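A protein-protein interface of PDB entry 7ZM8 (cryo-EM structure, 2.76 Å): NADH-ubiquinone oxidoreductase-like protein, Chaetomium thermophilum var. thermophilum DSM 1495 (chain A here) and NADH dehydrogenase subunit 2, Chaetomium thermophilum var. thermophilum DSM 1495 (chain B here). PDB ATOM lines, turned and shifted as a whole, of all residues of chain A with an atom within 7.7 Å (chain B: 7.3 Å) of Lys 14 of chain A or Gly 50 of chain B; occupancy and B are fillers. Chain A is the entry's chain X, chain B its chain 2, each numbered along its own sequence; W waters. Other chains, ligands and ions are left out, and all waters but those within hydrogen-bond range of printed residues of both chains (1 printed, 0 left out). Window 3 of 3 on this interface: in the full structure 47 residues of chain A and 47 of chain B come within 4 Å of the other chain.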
ATOM      1  N   TYR A   9      14.325  17.685  33.690  1.00  0.00           N
ATOM      2  CA  TYR A   9      13.223  17.505  32.709  1.00  0.00           C
ATOM      3  C   TYR A   9      13.739  16.480  31.699  1.00  0.00           C
ATOM      4  O   TYR A   9      14.621  16.836  30.898  1.00  0.00           O
ATOM      5  CB  TYR A   9      12.913  18.850  32.054  1.00  0.00           C
ATOM      6  CG  TYR A   9      11.637  18.950  31.260  1.00  0.00           C
ATOM      7  CD1 TYR A   9      11.613  18.662  29.906  1.00  0.00           C
ATOM      8  CD2 TYR A   9      10.463  19.386  31.851  1.00  0.00           C
ATOM      9  CE1 TYR A   9      10.449  18.778  29.164  1.00  0.00           C
ATOM     10  CE2 TYR A   9       9.290  19.502  31.125  1.00  0.00           C
ATOM     11  CZ  TYR A   9       9.284  19.197  29.776  1.00  0.00           C
ATOM     12  OH  TYR A   9       8.134  19.313  29.052  1.00  0.00           O
ATOM     13  N   PHE A  11      11.518  14.192  29.884  1.00  0.00           N
ATOM     14  CA  PHE A  11      10.507  13.706  28.910  1.00  0.00           C
ATOM     15  C   PHE A  11       9.727  14.882  28.298  1.00  0.00           C
ATOM     16  O   PHE A  11       9.395  15.794  29.067  1.00  0.00           O
ATOM     17  CB  PHE A  11       9.582  12.678  29.569  1.00  0.00           C
ATOM     18  CG  PHE A  11      10.286  11.547  30.274  1.00  0.00           C
ATOM     19  CD1 PHE A  11      10.520  11.596  31.638  1.00  0.00           C
ATOM     20  CD2 PHE A  11      10.721  10.434  29.573  1.00  0.00           C
ATOM     21  CE1 PHE A  11      11.175  10.560  32.284  1.00  0.00           C
ATOM     22  CE2 PHE A  11      11.375   9.398  30.219  1.00  0.00           C
ATOM     23  CZ  PHE A  11      11.598   9.461  31.574  1.00  0.00           C
ATOM     24  N   PRO A  12       9.371  14.906  26.984  1.00  0.00           N
ATOM     25  CA  PRO A  12       8.598  16.018  26.458  1.00  0.00           C
ATOM     26  C   PRO A  12       7.194  15.947  27.072  1.00  0.00           C
ATOM     27  O   PRO A  12       6.596  14.902  27.053  1.00  0.00           O
ATOM     28  CB  PRO A  12       8.654  15.798  24.937  1.00  0.00           C
ATOM     29  CG  PRO A  12       8.837  14.307  24.780  1.00  0.00           C
ATOM     30  CD  PRO A  12       9.651  13.878  25.982  1.00  0.00           C
ATOM     31  N   SER A  13       6.684  17.065  27.576  1.00  0.00           N
ATOM     32  CA  SER A  13       5.380  17.037  28.281  1.00  0.00           C
ATOM     33  C   SER A  13       4.496  18.140  27.726  1.00  0.00           C
ATOM     34  O   SER A  13       5.052  19.092  27.173  1.00  0.00           O
ATOM     35  CB  SER A  13       5.566  17.178  29.767  1.00  0.00           C
ATOM     36  OG  SER A  13       4.512  16.541  30.467  1.00  0.00           O
ATOM     37  N   LYS A  14       3.182  17.979  27.840  1.00  0.00           N
ATOM     38  CA  LYS A  14       2.236  19.020  27.365  1.00  0.00           C
ATOM     39  C   LYS A  14       2.105  20.136  28.397  1.00  0.00           C
ATOM     40  O   LYS A  14       1.833  19.817  29.557  1.00  0.00           O
ATOM     41  CB  LYS A  14       0.863  18.400  27.099  1.00  0.00           C
ATOM     42  CG  LYS A  14      -0.233  19.357  26.654  1.00  0.00           C
ATOM     43  CD  LYS A  14      -0.030  19.904  25.264  1.00  0.00           C
ATOM     44  CE  LYS A  14      -1.232  20.682  24.780  1.00  0.00           C
ATOM     45  NZ  LYS A  14      -1.004  21.278  23.443  1.00  0.00           N
ATOM     46  N   THR A  15       2.305  21.390  27.991  1.00  0.00           N
ATOM     47  CA  THR A  15       2.048  22.532  28.906  1.00  0.00           C
ATOM     48  C   THR A  15       0.593  22.963  28.692  1.00  0.00           C
ATOM     49  O   THR A  15       0.193  23.144  27.528  1.00  0.00           O
ATOM     50  CB  THR A  15       3.033  23.691  28.683  1.00  0.00           C
ATOM     51  OG1 THR A  15       4.314  23.293  29.165  1.00  0.00           O
ATOM     52  CG2 THR A  15       2.617  24.974  29.361  1.00  0.00           C
ATOM     53  N   VAL A  16      -0.165  23.079  29.778  1.00  0.00           N
ATOM     54  CA  VAL A  16      -1.572  23.540  29.678  1.00  0.00           C
ATOM     55  C   VAL A  16      -1.709  24.942  30.257  1.00  0.00           C
ATOM     56  O   VAL A  16      -1.120  25.191  31.312  1.00  0.00           O
ATOM     57  CB  VAL A  16      -2.561  22.543  30.299  1.00  0.00           C
ATOM     58  CG1 VAL A  16      -3.999  22.934  30.007  1.00  0.00           C
ATOM     59  CG2 VAL A  16      -2.292  21.132  29.812  1.00  0.00           C
ATOM     60  N   LYS A  17      -2.403  25.833  29.553  1.00  0.00           N
ATOM     61  CA  LYS A  17      -2.715  27.168  30.101  1.00  0.00           C
ATOM     62  C   LYS A  17      -3.721  27.060  31.248  1.00  0.00           C
ATOM     63  O   LYS A  17      -4.915  26.920  30.983  1.00  0.00           O
ATOM     64  CB  LYS A  17      -3.204  28.106  28.994  1.00  0.00           C
ATOM     65  CG  LYS A  17      -3.308  29.572  29.390  1.00  0.00           C
ATOM     66  CD  LYS A  17      -3.531  30.493  28.214  1.00  0.00           C
ATOM     67  CE  LYS A  17      -3.483  31.956  28.600  1.00  0.00           C
ATOM     68  NZ  LYS A  17      -2.211  32.299  29.280  1.00  0.00           N
ATOM     69  N   LEU A  22       1.427  24.052  38.320  1.00  0.00           N
ATOM     70  CA  LEU A  22       1.230  22.598  38.186  1.00  0.00           C
ATOM     71  C   LEU A  22       2.138  21.901  39.189  1.00  0.00           C
ATOM     72  O   LEU A  22       3.287  22.324  39.354  1.00  0.00           O
ATOM     73  CB  LEU A  22       1.571  22.168  36.758  1.00  0.00           C
ATOM     74  CG  LEU A  22       1.725  20.669  36.533  1.00  0.00           C
ATOM     75  CD1 LEU A  22       0.378  20.020  36.290  1.00  0.00           C
ATOM     76  CD2 LEU A  22       2.662  20.411  35.373  1.00  0.00           C
ATOM     77  N   ASN A  25       1.384  16.204  36.624  1.00  0.00           N
ATOM     78  CA  ASN A  25       0.501  15.965  35.453  1.00  0.00           C
ATOM     79  C   ASN A  25      -0.218  14.645  35.725  1.00  0.00           C
ATOM     80  O   ASN A  25      -1.291  14.420  35.139  1.00  0.00           O
ATOM     81  CB  ASN A  25       1.304  15.765  34.161  1.00  0.00           C
ATOM     82  CG  ASN A  25       1.598  17.034  33.400  1.00  0.00           C
ATOM     83  OD1 ASN A  25       1.298  18.121  33.871  1.00  0.00           O
ATOM     84  ND2 ASN A  25       2.184  16.904  32.222  1.00  0.00           N
ATOM     85  N   ARG A 144      -1.835  10.825  32.224  1.00  0.00           N
ATOM     86  CA  ARG A 144      -1.528  12.278  32.246  1.00  0.00           C
ATOM     87  C   ARG A 144      -2.822  13.061  31.959  1.00  0.00           C
ATOM     88  O   ARG A 144      -3.428  12.777  30.916  1.00  0.00           O
ATOM     89  CB  ARG A 144      -0.390  12.531  31.254  1.00  0.00           C
ATOM     90  CG  ARG A 144       0.393  13.815  31.479  1.00  0.00           C
ATOM     91  CD  ARG A 144       0.544  14.490  30.138  1.00  0.00           C
ATOM     92  NE  ARG A 144      -0.816  14.570  29.648  1.00  0.00           N
ATOM     93  CZ  ARG A 144      -1.184  14.541  28.380  1.00  0.00           C
ATOM     94  NH1 ARG A 144      -2.467  14.608  28.085  1.00  0.00           N
ATOM     95  NH2 ARG A 144      -0.288  14.436  27.419  1.00  0.00           N
ATOM     96  N   TYR A 145      -3.235  13.984  32.841  1.00  0.00           N
ATOM     97  CA  TYR A 145      -4.501  14.766  32.697  1.00  0.00           C
ATOM     98  C   TYR A 145      -5.726  13.880  32.429  1.00  0.00           C
ATOM     99  O   TYR A 145      -6.648  14.365  31.766  1.00  0.00           O
ATOM    100  CB  TYR A 145      -4.333  15.863  31.648  1.00  0.00           C
ATOM    101  CG  TYR A 145      -3.303  16.912  31.971  1.00  0.00           C
ATOM    102  CD1 TYR A 145      -3.409  17.695  33.107  1.00  0.00           C
ATOM    103  CD2 TYR A 145      -2.234  17.140  31.124  1.00  0.00           C
ATOM    104  CE1 TYR A 145      -2.468  18.665  33.403  1.00  0.00           C
ATOM    105  CE2 TYR A 145      -1.286  18.107  31.403  1.00  0.00           C
ATOM    106  CZ  TYR A 145      -1.406  18.877  32.545  1.00  0.00           C
ATOM    107  OH  TYR A 145      -0.477  19.837  32.820  1.00  0.00           O
ATOM    108  N   GLY A 165       5.580  15.771  34.398  1.00  0.00           N
ATOM    109  CA  GLY A 165       5.392  17.058  33.716  1.00  0.00           C
ATOM    110  C   GLY A 165       6.116  18.230  34.331  1.00  0.00           C
ATOM    111  O   GLY A 165       5.962  19.320  33.803  1.00  0.00           O
ATOM    112  N   PHE B  46      -9.242  25.133  32.025  1.00  0.00           N
ATOM    113  CA  PHE B  46      -8.003  25.313  31.293  1.00  0.00           C
ATOM    114  C   PHE B  46      -8.319  25.950  29.952  1.00  0.00           C
ATOM    115  O   PHE B  46      -9.448  25.893  29.466  1.00  0.00           O
ATOM    116  CB  PHE B  46      -7.265  23.981  31.097  1.00  0.00           C
ATOM    117  CG  PHE B  46      -8.069  22.944  30.366  1.00  0.00           C
ATOM    118  CD1 PHE B  46      -8.058  22.888  28.983  1.00  0.00           C
ATOM    119  CD2 PHE B  46      -8.837  22.030  31.061  1.00  0.00           C
ATOM    120  CE1 PHE B  46      -8.801  21.945  28.304  1.00  0.00           C
ATOM    121  CE2 PHE B  46      -9.575  21.084  30.390  1.00  0.00           C
ATOM    122  CZ  PHE B  46      -9.557  21.040  29.005  1.00  0.00           C
ATOM    123  N   ILE B  47      -7.325  26.593  29.353  1.00  0.00           N
ATOM    124  CA  ILE B  47      -7.481  27.182  27.998  1.00  0.00           C
ATOM    125  C   ILE B  47      -6.511  26.410  27.115  1.00  0.00           C
ATOM    126  O   ILE B  47      -5.305  26.537  27.306  1.00  0.00           O
ATOM    127  CB  ILE B  47      -7.168  28.684  28.008  1.00  0.00           C
ATOM    128  CG1 ILE B  47      -8.249  29.465  28.749  1.00  0.00           C
ATOM    129  CG2 ILE B  47      -6.992  29.202  26.591  1.00  0.00           C
ATOM    130  CD1 ILE B  47      -9.637  29.126  28.284  1.00  0.00           C
ATOM    131  N   SER B  48      -7.039  25.589  26.210  1.00  0.00           N
ATOM    132  CA  SER B  48      -6.151  24.720  25.403  1.00  0.00           C
ATOM    133  C   SER B  48      -6.824  24.413  24.079  1.00  0.00           C
ATOM    134  O   SER B  48      -8.033  24.131  24.086  1.00  0.00           O
ATOM    135  CB  SER B  48      -5.869  23.439  26.141  1.00  0.00           C
ATOM    136  OG  SER B  48      -5.032  22.586  25.376  1.00  0.00           O
ATOM    137  N   LYS B  49      -6.064  24.462  22.989  1.00  0.00           N
ATOM    138  CA  LYS B  49      -6.635  24.036  21.692  1.00  0.00           C
ATOM    139  C   LYS B  49      -6.947  22.542  21.820  1.00  0.00           C
ATOM    140  O   LYS B  49      -7.890  22.084  21.178  1.00  0.00           O
ATOM    141  CB  LYS B  49      -5.734  24.468  20.536  1.00  0.00           C
ATOM    142  CG  LYS B  49      -5.367  25.944  20.560  1.00  0.00           C
ATOM    143  CD  LYS B  49      -4.686  26.428  19.309  1.00  0.00           C
ATOM    144  CE  LYS B  49      -5.519  26.192  18.071  1.00  0.00           C
ATOM    145  NZ  LYS B  49      -5.185  27.162  17.002  1.00  0.00           N
ATOM    146  N   GLY B  50      -6.165  21.807  22.611  1.00  0.00           N
ATOM    147  CA  GLY B  50      -6.467  20.387  22.845  1.00  0.00           C
ATOM    148  C   GLY B  50      -5.395  19.676  23.644  1.00  0.00           C
ATOM    149  O   GLY B  50      -4.233  20.092  23.561  1.00  0.00           O
ATOM    150  N   ILE B  51      -5.782  18.655  24.412  1.00  0.00           N
ATOM    151  CA  ILE B  51      -4.803  17.839  25.179  1.00  0.00           C
ATOM    152  C   ILE B  51      -5.068  16.399  24.756  1.00  0.00           C
ATOM    153  O   ILE B  51      -6.216  16.033  24.755  1.00  0.00           O
ATOM    154  CB  ILE B  51      -4.945  18.032  26.703  1.00  0.00           C
ATOM    155  CG1 ILE B  51      -5.086  19.500  27.104  1.00  0.00           C
ATOM    156  CG2 ILE B  51      -3.807  17.350  27.439  1.00  0.00           C
ATOM    157  CD1 ILE B  51      -5.419  19.704  28.554  1.00  0.00           C
ATOM    158  N   GLY B  52      -4.043  15.643  24.383  1.00  0.00           N
ATOM    159  CA  GLY B  52      -4.175  14.243  23.978  1.00  0.00           C
ATOM    160  C   GLY B  52      -4.156  13.343  25.164  1.00  0.00           C
ATOM    161  O   GLY B  52      -3.247  13.464  25.956  1.00  0.00           O
ATOM    162  N   HIS B  59      -8.685  13.134  22.780  1.00  0.00           N
ATOM    163  CA  HIS B  59      -8.298  14.539  23.072  1.00  0.00           C
ATOM    164  C   HIS B  59      -9.409  15.205  23.870  1.00  0.00           C
ATOM    165  O   HIS B  59     -10.522  14.717  23.826  1.00  0.00           O
ATOM    166  CB  HIS B  59      -7.955  15.341  21.806  1.00  0.00           C
ATOM    167  CG  HIS B  59      -9.111  15.611  20.910  1.00  0.00           C
ATOM    168  ND1 HIS B  59      -9.915  16.719  21.055  1.00  0.00           N
ATOM    169  CD2 HIS B  59      -9.596  14.930  19.856  1.00  0.00           C
ATOM    170  CE1 HIS B  59     -10.854  16.698  20.136  1.00  0.00           C
ATOM    171  NE2 HIS B  59     -10.678  15.614  19.388  1.00  0.00           N
ATOM    172  N   ILE B  60      -9.093  16.261  24.602  1.00  0.00           N
ATOM    173  CA  ILE B  60     -10.107  17.068  25.333  1.00  0.00           C
ATOM    174  C   ILE B  60      -9.869  18.493  24.874  1.00  0.00           C
ATOM    175  O   ILE B  60      -8.704  18.863  24.722  1.00  0.00           O
ATOM    176  CB  ILE B  60      -9.971  16.962  26.862  1.00  0.00           C
ATOM    177  CG1 ILE B  60      -8.504  16.895  27.287  1.00  0.00           C
ATOM    178  CG2 ILE B  60     -10.766  15.783  27.395  1.00  0.00           C
ATOM    179  CD1 ILE B  60      -8.276  17.261  28.720  1.00  0.00           C
ATOM    180  N   THR B  61     -10.937  19.243  24.633  1.00  0.00           N
ATOM    181  CA  THR B  61     -10.868  20.660  24.209  1.00  0.00           C
ATOM    182  C   THR B  61     -11.975  21.321  25.007  1.00  0.00           C
ATOM    183  O   THR B  61     -12.810  20.582  25.523  1.00  0.00           O
ATOM    184  CB  THR B  61     -11.050  20.775  22.685  1.00  0.00           C
ATOM    185  OG1 THR B  61     -10.023  20.052  22.005  1.00  0.00           O
ATOM    186  CG2 THR B  61     -11.075  22.195  22.173  1.00  0.00           C
ATOM    187  N   ASN B  62     -11.964  22.635  25.121  1.00  0.00           N
ATOM    188  CA  ASN B  62     -13.057  23.357  25.802  1.00  0.00           C
ATOM    189  C   ASN B  62     -14.327  23.052  25.009  1.00  0.00           C
ATOM    190  O   ASN B  62     -15.341  22.784  25.630  1.00  0.00           O
ATOM    191  CB  ASN B  62     -12.681  24.828  25.956  1.00  0.00           C
ATOM    192  CG  ASN B  62     -11.628  25.066  27.012  1.00  0.00           C
ATOM    193  OD1 ASN B  62     -11.937  25.089  28.200  1.00  0.00           O
ATOM    194  ND2 ASN B  62     -10.391  25.260  26.589  1.00  0.00           N
ATOM    195  N   ASP B 207      -3.140  14.685  14.141  1.00  0.00           N
ATOM    196  CA  ASP B 207      -2.104  15.742  14.250  1.00  0.00           C
ATOM    197  C   ASP B 207      -0.962  15.542  13.255  1.00  0.00           C
ATOM    198  O   ASP B 207      -0.529  16.555  12.700  1.00  0.00           O
ATOM    199  CB  ASP B 207      -1.601  15.857  15.686  1.00  0.00           C
ATOM    200  CG  ASP B 207      -2.466  16.783  16.529  1.00  0.00           C
ATOM    201  OD1 ASP B 207      -1.979  17.263  17.572  1.00  0.00           O
ATOM    202  OD2 ASP B 207      -3.624  17.021  16.135  1.00  0.00           O
ATOM    203  N   TYR B 297      -8.232  22.557  10.538  1.00  0.00           N
ATOM    204  CA  TYR B 297      -6.797  22.209  10.386  1.00  0.00           C
ATOM    205  C   TYR B 297      -6.532  21.631   9.006  1.00  0.00           C
ATOM    206  O   TYR B 297      -5.399  21.205   8.782  1.00  0.00           O
ATOM    207  CB  TYR B 297      -6.360  21.193  11.436  1.00  0.00           C
ATOM    208  CG  TYR B 297      -6.383  21.647  12.871  1.00  0.00           C
ATOM    209  CD1 TYR B 297      -5.379  22.449  13.382  1.00  0.00           C
ATOM    210  CD2 TYR B 297      -7.385  21.235  13.729  1.00  0.00           C
ATOM    211  CE1 TYR B 297      -5.388  22.854  14.706  1.00  0.00           C
ATOM    212  CE2 TYR B 297      -7.412  21.632  15.053  1.00  0.00           C
ATOM    213  CZ  TYR B 297      -6.409  22.445  15.544  1.00  0.00           C
ATOM    214  OH  TYR B 297      -6.424  22.842  16.848  1.00  0.00           O
ATOM    215  N   ILE B 567     -10.324  30.540  21.097  1.00  0.00           N
ATOM    216  CA  ILE B 567      -9.296  29.511  21.432  1.00  0.00           C
ATOM    217  C   ILE B 567      -8.932  28.683  20.198  1.00  0.00           C
ATOM    218  O   ILE B 567      -7.751  28.459  19.973  1.00  0.00           O
ATOM    219  CB  ILE B 567      -9.746  28.640  22.623  1.00  0.00           C
ATOM    220  CG1 ILE B 567     -10.154  29.485  23.832  1.00  0.00           C
ATOM    221  CG2 ILE B 567      -8.694  27.611  22.990  1.00  0.00           C
ATOM    222  CD1 ILE B 567     -10.972  28.731  24.853  1.00  0.00           C
HETATM  223  O   HOH W   1      -2.491  23.901  26.221  1.00  0.00           O
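O of Gly 50 of chain B sits close to NZ of Lys 14 of chain A, at 3.4 Å. N of Ile 47 of chain B is in hydrogen-bond range of O of Lys 17 of chain A (2.9 Å). O of Gly 52 of chain B lies within hydrogen-bond range of NH1 of Arg 144 of chain A (2.5 Å).
The side-chain amide oxygen of Asn 62 of chain B sits close to the backbone carbonyl oxygen of Phe 46 of chain B (2.9 Å). OG of Ser 48 of chain B sits close to N of Gly 50 of chain B. The backbone NH of Ile 60 of chain B sits at hydrogen-bond distance from the backbone carbonyl oxygen of Ile 51 of chain B (2.9 Å).
Among the printed residues, merely in contact across the chains: Val 16 of chain A with Phe 46 of chain B (3.6 Å), Val 16 of chain A with Ile 51 of chain B (3.7 Å), Lys 17 of chain A with Phe 46 of chain B (3.5 Å) and Arg 144 of chain A with Ile 51 of chain B (3.1 Å).
Lys 14 of chain A touches just one residue of chain B: Gly 50. Printed residues of chain B within 4 Å of Val 16 of chain A: Phe 46 and Ile 51. Of the printed residues of chain B, Arg 144 of chain A touches Ile 51 (3.1 Å) and Gly 52 (2.5 Å). Printed residues of chain A within 4 Å of Phe 46 of chain B: Val 16 and Lys 17. Of the printed residues of chain A, Ile 47 of chain B touches Lys 17. Lys 49 of chain B touches none of the printed residues of chain A. The nearest residue of chain B that does not touch Lys 14 of chain A is Ile 51 of chain B (4.2 Å). The nearest residue of chain A that does not touch Gly 50 of chain B is Val 16 of chain A (6.6 Å).
Hydrophobic or aromatic side chains of chain A that line the printed part of chain B: Val 16. Hydrophobic or aromatic side chains of chain B that line the printed part of chain A: Phe 46 and Ile 51. Along chain B the printed residues that touch a printed residue of chain A span positions 46 to 52. Among the printed residues, 7 pairs touch across the chains.
Water W1 bridges the side-chain hydroxyl (OG) of Ser 48 of chain B (3.0 Å) and the backbone carbonyl oxygen (O) of Thr 15 of chain A (3.1 Å).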
